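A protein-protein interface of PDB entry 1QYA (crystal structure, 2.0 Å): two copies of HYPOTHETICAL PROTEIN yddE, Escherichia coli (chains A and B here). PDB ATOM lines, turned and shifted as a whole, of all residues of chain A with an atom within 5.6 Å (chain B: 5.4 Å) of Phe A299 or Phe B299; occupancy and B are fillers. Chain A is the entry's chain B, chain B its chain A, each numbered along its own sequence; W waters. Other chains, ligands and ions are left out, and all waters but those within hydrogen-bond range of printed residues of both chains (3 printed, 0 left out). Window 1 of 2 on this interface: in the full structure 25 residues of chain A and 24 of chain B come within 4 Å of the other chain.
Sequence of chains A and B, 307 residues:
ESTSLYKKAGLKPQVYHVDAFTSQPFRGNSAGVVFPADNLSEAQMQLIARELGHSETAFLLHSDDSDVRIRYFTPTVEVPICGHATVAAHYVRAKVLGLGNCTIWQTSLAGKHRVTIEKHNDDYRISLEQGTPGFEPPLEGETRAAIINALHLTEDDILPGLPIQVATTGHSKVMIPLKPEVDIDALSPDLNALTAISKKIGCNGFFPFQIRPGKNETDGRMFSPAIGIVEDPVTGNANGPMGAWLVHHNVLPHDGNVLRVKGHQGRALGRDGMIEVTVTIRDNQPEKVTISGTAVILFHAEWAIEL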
ATOM      1  N   VAL A  15      -7.000  18.586 -23.433  1.00  0.00           N
ATOM      2  CA  VAL A  15      -5.743  18.025 -23.894  1.00  0.00           C
ATOM      3  C   VAL A  15      -4.633  19.031 -23.553  1.00  0.00           C
ATOM      4  O   VAL A  15      -4.808  20.225 -23.721  1.00  0.00           O
ATOM      5  CB  VAL A  15      -5.790  17.718 -25.418  1.00  0.00           C
ATOM      6  CG1 VAL A  15      -6.222  18.931 -26.219  1.00  0.00           C
ATOM      7  CG2 VAL A  15      -4.439  17.232 -25.894  1.00  0.00           C
ATOM      8  N   TYR A  16      -3.511  18.524 -23.048  1.00  0.00           N
ATOM      9  CA  TYR A  16      -2.278  19.275 -22.821  1.00  0.00           C
ATOM     10  C   TYR A  16      -1.199  18.676 -23.711  1.00  0.00           C
ATOM     11  O   TYR A  16      -1.085  17.450 -23.829  1.00  0.00           O
ATOM     12  CB  TYR A  16      -1.844  19.171 -21.364  1.00  0.00           C
ATOM     13  CG  TYR A  16      -2.833  19.785 -20.392  1.00  0.00           C
ATOM     14  CD1 TYR A  16      -3.987  19.104 -19.996  1.00  0.00           C
ATOM     15  CD2 TYR A  16      -2.628  21.043 -19.891  1.00  0.00           C
ATOM     16  CE1 TYR A  16      -4.896  19.691 -19.119  1.00  0.00           C
ATOM     17  CE2 TYR A  16      -3.519  21.627 -19.010  1.00  0.00           C
ATOM     18  CZ  TYR A  16      -4.652  20.961 -18.638  1.00  0.00           C
ATOM     19  OH  TYR A  16      -5.533  21.588 -17.775  1.00  0.00           O
ATOM     20  N   HIS A  17      -0.429  19.528 -24.365  1.00  0.00           N
ATOM     21  CA  HIS A  17       0.730  19.081 -25.122  1.00  0.00           C
ATOM     22  C   HIS A  17       1.976  19.518 -24.336  1.00  0.00           C
ATOM     23  O   HIS A  17       2.198  20.692 -24.095  1.00  0.00           O
ATOM     24  CB  HIS A  17       0.685  19.632 -26.539  1.00  0.00           C
ATOM     25  CG  HIS A  17       1.846  19.227 -27.388  1.00  0.00           C
ATOM     26  ND1 HIS A  17       1.737  19.063 -28.747  1.00  0.00           N
ATOM     27  CD2 HIS A  17       3.145  18.996 -27.088  1.00  0.00           C
ATOM     28  CE1 HIS A  17       2.912  18.728 -29.247  1.00  0.00           C
ATOM     29  NE2 HIS A  17       3.785  18.685 -28.259  1.00  0.00           N
ATOM     30  N   LEU A  52      -3.219  12.082 -31.320  1.00  0.00           N
ATOM     31  CA  LEU A  52      -2.209  13.034 -30.846  1.00  0.00           C
ATOM     32  C   LEU A  52      -0.805  12.658 -31.342  1.00  0.00           C
ATOM     33  O   LEU A  52       0.013  13.526 -31.617  1.00  0.00           O
ATOM     34  CB  LEU A  52      -2.229  13.155 -29.312  1.00  0.00           C
ATOM     35  CG  LEU A  52      -3.517  13.725 -28.723  1.00  0.00           C
ATOM     36  CD1 LEU A  52      -3.413  13.797 -27.228  1.00  0.00           C
ATOM     37  CD2 LEU A  52      -3.822  15.126 -29.298  1.00  0.00           C
ATOM     38  N   ILE A 297       4.434  23.133 -20.625  1.00  0.00           N
ATOM     39  CA  ILE A 297       3.163  23.012 -21.352  1.00  0.00           C
ATOM     40  C   ILE A 297       3.166  23.970 -22.537  1.00  0.00           C
ATOM     41  O   ILE A 297       3.196  25.177 -22.350  1.00  0.00           O
ATOM     42  CB  ILE A 297       1.987  23.347 -20.410  1.00  0.00           C
ATOM     43  CG1 ILE A 297       1.891  22.301 -19.305  1.00  0.00           C
ATOM     44  CG2 ILE A 297       0.677  23.410 -21.169  1.00  0.00           C
ATOM     45  CD1 ILE A 297       1.166  22.841 -18.061  1.00  0.00           C
ATOM     46  N   LEU A 298       3.156  23.428 -23.751  1.00  0.00           N
ATOM     47  CA  LEU A 298       3.112  24.262 -24.950  1.00  0.00           C
ATOM     48  C   LEU A 298       1.746  24.900 -25.174  1.00  0.00           C
ATOM     49  O   LEU A 298       1.657  26.028 -25.608  1.00  0.00           O
ATOM     50  CB  LEU A 298       3.494  23.446 -26.183  1.00  0.00           C
ATOM     51  CG  LEU A 298       4.833  22.713 -26.146  1.00  0.00           C
ATOM     52  CD1 LEU A 298       5.226  22.224 -27.544  1.00  0.00           C
ATOM     53  CD2 LEU A 298       5.894  23.615 -25.593  1.00  0.00           C
ATOM     54  N   PHE A 299       0.689  24.131 -24.932  1.00  0.00           N
ATOM     55  CA  PHE A 299      -0.677  24.633 -24.997  1.00  0.00           C
ATOM     56  C   PHE A 299      -1.645  23.616 -24.423  1.00  0.00           C
ATOM     57  O   PHE A 299      -1.329  22.411 -24.253  1.00  0.00           O
ATOM     58  CB  PHE A 299      -1.099  24.941 -26.444  1.00  0.00           C
ATOM     59  CG  PHE A 299      -0.976  23.774 -27.367  1.00  0.00           C
ATOM     60  CD1 PHE A 299      -1.966  22.809 -27.419  1.00  0.00           C
ATOM     61  CD2 PHE A 299       0.130  23.637 -28.191  1.00  0.00           C
ATOM     62  CE1 PHE A 299      -1.856  21.731 -28.274  1.00  0.00           C
ATOM     63  CE2 PHE A 299       0.243  22.560 -29.059  1.00  0.00           C
ATOM     64  CZ  PHE A 299      -0.741  21.605 -29.094  1.00  0.00           C
ATOM     65  N   HIS A 300      -2.839  24.096 -24.150  1.00  0.00           N
ATOM     66  CA  HIS A 300      -3.898  23.232 -23.644  1.00  0.00           C
ATOM     67  C   HIS A 300      -5.249  23.787 -24.065  1.00  0.00           C
ATOM     68  O   HIS A 300      -5.383  24.985 -24.262  1.00  0.00           O
ATOM     69  CB  HIS A 300      -3.789  23.065 -22.118  1.00  0.00           C
ATOM     70  CG  HIS A 300      -4.067  24.313 -21.346  1.00  0.00           C
ATOM     71  ND1 HIS A 300      -5.332  24.661 -20.925  1.00  0.00           N
ATOM     72  CD2 HIS A 300      -3.242  25.293 -20.907  1.00  0.00           C
ATOM     73  CE1 HIS A 300      -5.275  25.813 -20.277  1.00  0.00           C
ATOM     74  NE2 HIS A 300      -4.016  26.212 -20.248  1.00  0.00           N
ATOM     75  N   ALA A 301      -6.232  22.904 -24.228  1.00  0.00           N
ATOM     76  CA  ALA A 301      -7.616  23.332 -24.481  1.00  0.00           C
ATOM     77  C   ALA A 301      -8.637  22.212 -24.262  1.00  0.00           C
ATOM     78  O   ALA A 301      -8.314  21.026 -24.299  1.00  0.00           O
ATOM     79  CB  ALA A 301      -7.742  23.870 -25.903  1.00  0.00           C
ATOM     80  N   GLU A 302      -9.877  22.622 -24.016  1.00  0.00           N
ATOM     81  CA  GLU A 302     -11.017  21.724 -24.088  1.00  0.00           C
ATOM     82  C   GLU A 302     -11.131  21.277 -25.537  1.00  0.00           C
ATOM     83  O   GLU A 302     -10.676  21.964 -26.453  1.00  0.00           O
ATOM     84  CB  GLU A 302     -12.313  22.436 -23.682  1.00  0.00           C
ATOM     85  CG  GLU A 302     -12.403  22.891 -22.227  1.00  0.00           C
ATOM     86  CD  GLU A 302     -13.640  23.741 -21.945  1.00  0.00           C
ATOM     87  OE1 GLU A 302     -14.359  24.102 -22.890  1.00  0.00           O
ATOM     88  OE2 GLU A 302     -13.908  24.051 -20.778  1.00  0.00           O
ATOM     89  N   TRP A 303     -11.728  20.112 -25.729  1.00  0.00           N
ATOM     90  CA  TRP A 303     -12.052  19.586 -27.060  1.00  0.00           C
ATOM     91  C   TRP A 303     -13.235  20.342 -27.654  1.00  0.00           C
ATOM     92  O   TRP A 303     -14.113  20.797 -26.920  1.00  0.00           O
ATOM     93  CB  TRP A 303     -12.368  18.094 -26.962  1.00  0.00           C
ATOM     94  CG  TRP A 303     -11.168  17.296 -26.594  1.00  0.00           C
ATOM     95  CD1 TRP A 303     -10.627  17.154 -25.353  1.00  0.00           C
ATOM     96  CD2 TRP A 303     -10.333  16.543 -27.478  1.00  0.00           C
ATOM     97  NE1 TRP A 303      -9.500  16.372 -25.404  1.00  0.00           N
ATOM     98  CE2 TRP A 303      -9.302  15.973 -26.699  1.00  0.00           C
ATOM     99  CE3 TRP A 303     -10.351  16.291 -28.843  1.00  0.00           C
ATOM    100  CZ2 TRP A 303      -8.311  15.166 -27.244  1.00  0.00           C
ATOM    101  CZ3 TRP A 303      -9.373  15.495 -29.381  1.00  0.00           C
ATOM    102  CH2 TRP A 303      -8.361  14.941 -28.583  1.00  0.00           C
ATOM    103  N   ALA A 304     -13.234  20.526 -28.972  1.00  0.00           N
ATOM    104  CA  ALA A 304     -14.331  21.215 -29.660  1.00  0.00           C
ATOM    105  C   ALA A 304     -15.439  20.241 -30.017  1.00  0.00           C
ATOM    106  O   ALA A 304     -16.521  20.646 -30.402  1.00  0.00           O
ATOM    107  CB  ALA A 304     -13.825  21.899 -30.910  1.00  0.00           C
ATOM    108  N   VAL B  15      -3.205  27.206 -32.446  1.00  0.00           N
ATOM    109  CA  VAL B  15      -2.963  25.956 -33.119  1.00  0.00           C
ATOM    110  C   VAL B  15      -4.286  25.181 -33.212  1.00  0.00           C
ATOM    111  O   VAL B  15      -5.011  25.078 -32.237  1.00  0.00           O
ATOM    112  CB  VAL B  15      -1.863  25.130 -32.414  1.00  0.00           C
ATOM    113  CG1 VAL B  15      -2.216  24.867 -30.965  1.00  0.00           C
ATOM    114  CG2 VAL B  15      -1.642  23.840 -33.170  1.00  0.00           C
ATOM    115  N   TYR B  16      -4.588  24.668 -34.393  1.00  0.00           N
ATOM    116  CA  TYR B  16      -5.793  23.894 -34.637  1.00  0.00           C
ATOM    117  C   TYR B  16      -5.368  22.503 -35.009  1.00  0.00           C
ATOM    118  O   TYR B  16      -4.455  22.315 -35.822  1.00  0.00           O
ATOM    119  CB  TYR B  16      -6.639  24.495 -35.769  1.00  0.00           C
ATOM    120  CG  TYR B  16      -7.256  25.833 -35.438  1.00  0.00           C
ATOM    121  CD1 TYR B  16      -6.480  26.990 -35.416  1.00  0.00           C
ATOM    122  CD2 TYR B  16      -8.616  25.952 -35.152  1.00  0.00           C
ATOM    123  CE1 TYR B  16      -7.033  28.223 -35.100  1.00  0.00           C
ATOM    124  CE2 TYR B  16      -9.180  27.187 -34.822  1.00  0.00           C
ATOM    125  CZ  TYR B  16      -8.381  28.312 -34.804  1.00  0.00           C
ATOM    126  OH  TYR B  16      -8.917  29.542 -34.511  1.00  0.00           O
ATOM    127  N   HIS B  17      -6.044  21.527 -34.428  1.00  0.00           N
ATOM    128  CA  HIS B  17      -5.887  20.151 -34.826  1.00  0.00           C
ATOM    129  C   HIS B  17      -7.140  19.774 -35.624  1.00  0.00           C
ATOM    130  O   HIS B  17      -8.255  19.798 -35.097  1.00  0.00           O
ATOM    131  CB  HIS B  17      -5.707  19.269 -33.595  1.00  0.00           C
ATOM    132  CG  HIS B  17      -5.362  17.858 -33.925  1.00  0.00           C
ATOM    133  ND1 HIS B  17      -4.326  17.187 -33.313  1.00  0.00           N
ATOM    134  CD2 HIS B  17      -5.914  16.987 -34.801  1.00  0.00           C
ATOM    135  CE1 HIS B  17      -4.268  15.954 -33.789  1.00  0.00           C
ATOM    136  NE2 HIS B  17      -5.214  15.812 -34.701  1.00  0.00           N
ATOM    137  N   LEU B  52       4.199  19.177 -33.581  1.00  0.00           N
ATOM    138  CA  LEU B  52       2.826  18.707 -33.702  1.00  0.00           C
ATOM    139  C   LEU B  52       2.752  17.305 -34.327  1.00  0.00           C
ATOM    140  O   LEU B  52       1.830  16.551 -34.043  1.00  0.00           O
ATOM    141  CB  LEU B  52       1.962  19.699 -34.487  1.00  0.00           C
ATOM    142  CG  LEU B  52       1.853  21.117 -33.917  1.00  0.00           C
ATOM    143  CD1 LEU B  52       1.085  22.031 -34.870  1.00  0.00           C
ATOM    144  CD2 LEU B  52       1.207  21.115 -32.542  1.00  0.00           C
ATOM    145  N   ILE B 297     -12.689  20.288 -36.765  1.00  0.00           N
ATOM    146  CA  ILE B 297     -11.709  20.771 -35.792  1.00  0.00           C
ATOM    147  C   ILE B 297     -11.891  20.013 -34.494  1.00  0.00           C
ATOM    148  O   ILE B 297     -12.932  20.114 -33.858  1.00  0.00           O
ATOM    149  CB  ILE B 297     -11.907  22.289 -35.556  1.00  0.00           C
ATOM    150  CG1 ILE B 297     -11.560  23.089 -36.832  1.00  0.00           C
ATOM    151  CG2 ILE B 297     -11.073  22.778 -34.374  1.00  0.00           C
ATOM    152  CD1 ILE B 297     -12.149  24.496 -36.820  1.00  0.00           C
ATOM    153  N   LEU B 298     -10.891  19.228 -34.100  1.00  0.00           N
ATOM    154  CA  LEU B 298     -10.956  18.506 -32.818  1.00  0.00           C
ATOM    155  C   LEU B 298     -10.750  19.397 -31.597  1.00  0.00           C
ATOM    156  O   LEU B 298     -11.361  19.180 -30.533  1.00  0.00           O
ATOM    157  CB  LEU B 298      -9.909  17.398 -32.791  1.00  0.00           C
ATOM    158  CG  LEU B 298      -9.920  16.429 -33.963  1.00  0.00           C
ATOM    159  CD1 LEU B 298      -9.086  15.212 -33.623  1.00  0.00           C
ATOM    160  CD2 LEU B 298     -11.330  16.011 -34.335  1.00  0.00           C
ATOM    161  N   PHE B 299      -9.846  20.357 -31.744  1.00  0.00           N
ATOM    162  CA  PHE B 299      -9.569  21.373 -30.729  1.00  0.00           C
ATOM    163  C   PHE B 299      -8.693  22.479 -31.300  1.00  0.00           C
ATOM    164  O   PHE B 299      -8.072  22.319 -32.338  1.00  0.00           O
ATOM    165  CB  PHE B 299      -8.893  20.789 -29.467  1.00  0.00           C
ATOM    166  CG  PHE B 299      -7.547  20.135 -29.724  1.00  0.00           C
ATOM    167  CD1 PHE B 299      -6.376  20.884 -29.686  1.00  0.00           C
ATOM    168  CD2 PHE B 299      -7.455  18.763 -29.981  1.00  0.00           C
ATOM    169  CE1 PHE B 299      -5.135  20.286 -29.913  1.00  0.00           C
ATOM    170  CE2 PHE B 299      -6.212  18.158 -30.193  1.00  0.00           C
ATOM    171  CZ  PHE B 299      -5.054  18.935 -30.172  1.00  0.00           C
ATOM    172  N   HIS B 300      -8.668  23.608 -30.605  1.00  0.00           N
ATOM    173  CA  HIS B 300      -7.742  24.685 -30.898  1.00  0.00           C
ATOM    174  C   HIS B 300      -7.356  25.391 -29.613  1.00  0.00           C
ATOM    175  O   HIS B 300      -8.151  25.449 -28.675  1.00  0.00           O
ATOM    176  CB  HIS B 300      -8.358  25.688 -31.891  1.00  0.00           C
ATOM    177  CG  HIS B 300      -9.619  26.340 -31.407  1.00  0.00           C
ATOM    178  ND1 HIS B 300      -9.640  27.597 -30.846  1.00  0.00           N
ATOM    179  CD2 HIS B 300     -10.911  25.926 -31.448  1.00  0.00           C
ATOM    180  CE1 HIS B 300     -10.882  27.915 -30.520  1.00  0.00           C
ATOM    181  NE2 HIS B 300     -11.675  26.925 -30.888  1.00  0.00           N
ATOM    182  N   ALA B 301      -6.142  25.936 -29.579  1.00  0.00           N
ATOM    183  CA  ALA B 301      -5.655  26.671 -28.404  1.00  0.00           C
ATOM    184  C   ALA B 301      -4.677  27.780 -28.760  1.00  0.00           C
ATOM    185  O   ALA B 301      -3.970  27.710 -29.760  1.00  0.00           O
ATOM    186  CB  ALA B 301      -4.974  25.713 -27.444  1.00  0.00           C
ATOM    187  N   GLU B 302      -4.624  28.791 -27.899  1.00  0.00           N
ATOM    188  CA  GLU B 302      -3.536  29.760 -27.906  1.00  0.00           C
ATOM    189  C   GLU B 302      -2.285  29.073 -27.394  1.00  0.00           C
ATOM    190  O   GLU B 302      -2.353  28.253 -26.471  1.00  0.00           O
ATOM    191  CB  GLU B 302      -3.854  30.957 -27.011  1.00  0.00           C
ATOM    192  CG  GLU B 302      -5.054  31.756 -27.482  1.00  0.00           C
ATOM    193  CD  GLU B 302      -5.332  32.978 -26.628  1.00  0.00           C
ATOM    194  OE1 GLU B 302      -4.507  33.311 -25.738  1.00  0.00           O
ATOM    195  OE2 GLU B 302      -6.385  33.611 -26.864  1.00  0.00           O
ATOM    196  N   TRP B 303      -1.150  29.394 -28.006  1.00  0.00           N
ATOM    197  CA  TRP B 303       0.128  28.897 -27.526  1.00  0.00           C
ATOM    198  C   TRP B 303       0.343  29.483 -26.125  1.00  0.00           C
ATOM    199  O   TRP B 303       0.154  30.668 -25.920  1.00  0.00           O
ATOM    200  CB  TRP B 303       1.271  29.266 -28.493  1.00  0.00           C
ATOM    201  CG  TRP B 303       1.206  28.503 -29.786  1.00  0.00           C
ATOM    202  CD1 TRP B 303       0.523  28.861 -30.909  1.00  0.00           C
ATOM    203  CD2 TRP B 303       1.813  27.235 -30.079  1.00  0.00           C
ATOM    204  NE1 TRP B 303       0.665  27.905 -31.886  1.00  0.00           N
ATOM    205  CE2 TRP B 303       1.466  26.900 -31.411  1.00  0.00           C
ATOM    206  CE3 TRP B 303       2.633  26.356 -29.362  1.00  0.00           C
ATOM    207  CZ2 TRP B 303       1.896  25.715 -32.032  1.00  0.00           C
ATOM    208  CZ3 TRP B 303       3.082  25.190 -29.986  1.00  0.00           C
ATOM    209  CH2 TRP B 303       2.704  24.878 -31.307  1.00  0.00           C
ATOM    210  N   ALA B 304       0.678  28.629 -25.157  1.00  0.00           N
ATOM    211  CA  ALA B 304       0.955  29.060 -23.775  1.00  0.00           C
ATOM    212  C   ALA B 304       2.416  29.497 -23.579  1.00  0.00           C
ATOM    213  O   ALA B 304       2.821  29.863 -22.477  1.00  0.00           O
ATOM    214  CB  ALA B 304       0.604  27.938 -22.784  1.00  0.00           C
HETATM  215  O   HOH W   1     -11.004  23.566 -28.493  1.00  0.00           O
HETATM  216  O   HOH W   2      -2.965  27.175 -24.137  1.00  0.00           O
HETATM  217  O   HOH W   3       2.863  13.962 -32.581  1.00  0.00           O
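The backbone NH of Ala A304 sits at hydrogen-bond distance from the backbone carbonyl oxygen of Leu B298 (2.8 Å).
N of Ala B304 is in hydrogen-bond range of O of Leu A298.
The backbone carbonyl oxygen of Ala B301 lies within hydrogen-bond range of the backbone NH of Val B15.
The backbone NH (N) of Leu B298 sits at hydrogen-bond distance from the backbone carbonyl oxygen (O) of His B17.
N of His B17 sits at hydrogen-bond distance from O of Phe B299 (3.0 Å).
The backbone carbonyl oxygen (O) of Ala A301 is in hydrogen-bond range of the backbone NH (N) of Val A15 (2.9 Å).
N of Leu A298 is in hydrogen-bond range of O of His A17 (2.9 Å).
N of His A17 is in hydrogen-bond range of O of Phe A299 (3.0 Å).
Among the printed residues, pairs that only touch across the chains: Ala A301 with His B300 (3.2 Å), His A300 with Ala B301 (3.3 Å), Trp A303 with Leu B298 (3.5 Å), Phe A299 with Glu B302 (3.5 Å), Ala A304 with Ile B297 (3.6 Å), Ala A301 with Ala B301 (3.7 Å), Glu A302 with Phe B299 (3.7 Å), Leu A298 with Trp B303 (3.7 Å), Phe A299 with Trp B303 (3.8 Å), Ile A297 with Ala B304 (3.8 Å), Phe A299 with Val B15 (3.8 Å), Trp A303 with Phe B299 (3.8 Å), Phe A299 with Leu B52 (3.9 Å), Val A15 with Phe B299 (3.9 Å), Phe A299 with Phe B299 (3.9 Å) and Leu A52 with Phe B299 (3.96 Å).
Printed residues of chain B within 4 Å of Val A15: Phe B299 (3.9 Å).
His A17 touches none of the printed residues of chain B.
Printed residues of chain B within 4 Å of Leu A52: Phe B299.
Phe A299 touches just these residues of chain B: Val B15 (3.8 Å), Leu B52 (3.9 Å), Phe B299 (3.9 Å), Glu B302 (3.5 Å) and Trp B303 (3.8 Å).
Of the printed residues of chain A, Val B15 touches Phe A299 (3.8 Å).
Phe B299 touches five residues of chain A.
Of the printed residues of chain A, Glu B302 touches Phe A299.
Printed residues of chain A within 4 Å of Ala B304: Ile A297 and Leu A298.
The nearest residue of chain B that does not touch Phe A299 is Ala B301 (4.1 Å).
The nearest residue of chain A that does not touch Phe B299 is Ala A304 (4.2 Å).
The nearest printed residue of chain A that does not touch Glu B302 is Leu A298 (4.7 Å).
Of the 12 printed residues of chain B, 10 touch a printed residue of chain A.
Hydrophobic or aromatic side chains of chain B that line the printed part of chain A: Val B15, Leu B52, Leu B298, Phe B299, Ala B301, Trp B303 and Ala B304.
Hydrophobic or aromatic side chains of chain A that line the printed part of chain B: Val A15, Leu A52, Phe A299, Ala A301, Trp A303 and Ala A304.
Among the printed residues, 18 pairs touch across the chains.
Among the printed residues, no Asp or Glu carboxylate lies within 4 Å of a Lys or Arg side-chain nitrogen of the other chain.
Val A15 touches Phe B299, and with the chains exchanged Phe A299 touches Val B15.
Leu A52 touches Phe B299, and with the chains exchanged Phe A299 touches Leu B52.
Ile A297 touches Ala B304, and with the chains exchanged Ala A304 touches Ile B297.
Phe A299 touches Trp B303, and with the chains exchanged Trp A303 touches Phe B299.
12 positions are printed for both chains.
Of the 18 pairs that touch across the chains among the printed residues, 18 have their exchanged pair printed and touching as well.
Water W1 bridges O of Glu A302 (2.6 Å) and N of His B300 (3.1 Å).
Water W2 lies within hydrogen-bond range of the backbone carbonyl oxygen (O) of Glu B302 and the backbone NH (N) of His A300.
Water W3 bridges O of Leu A52 (3.0 Å) and O of Leu B52 (3.1 Å).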
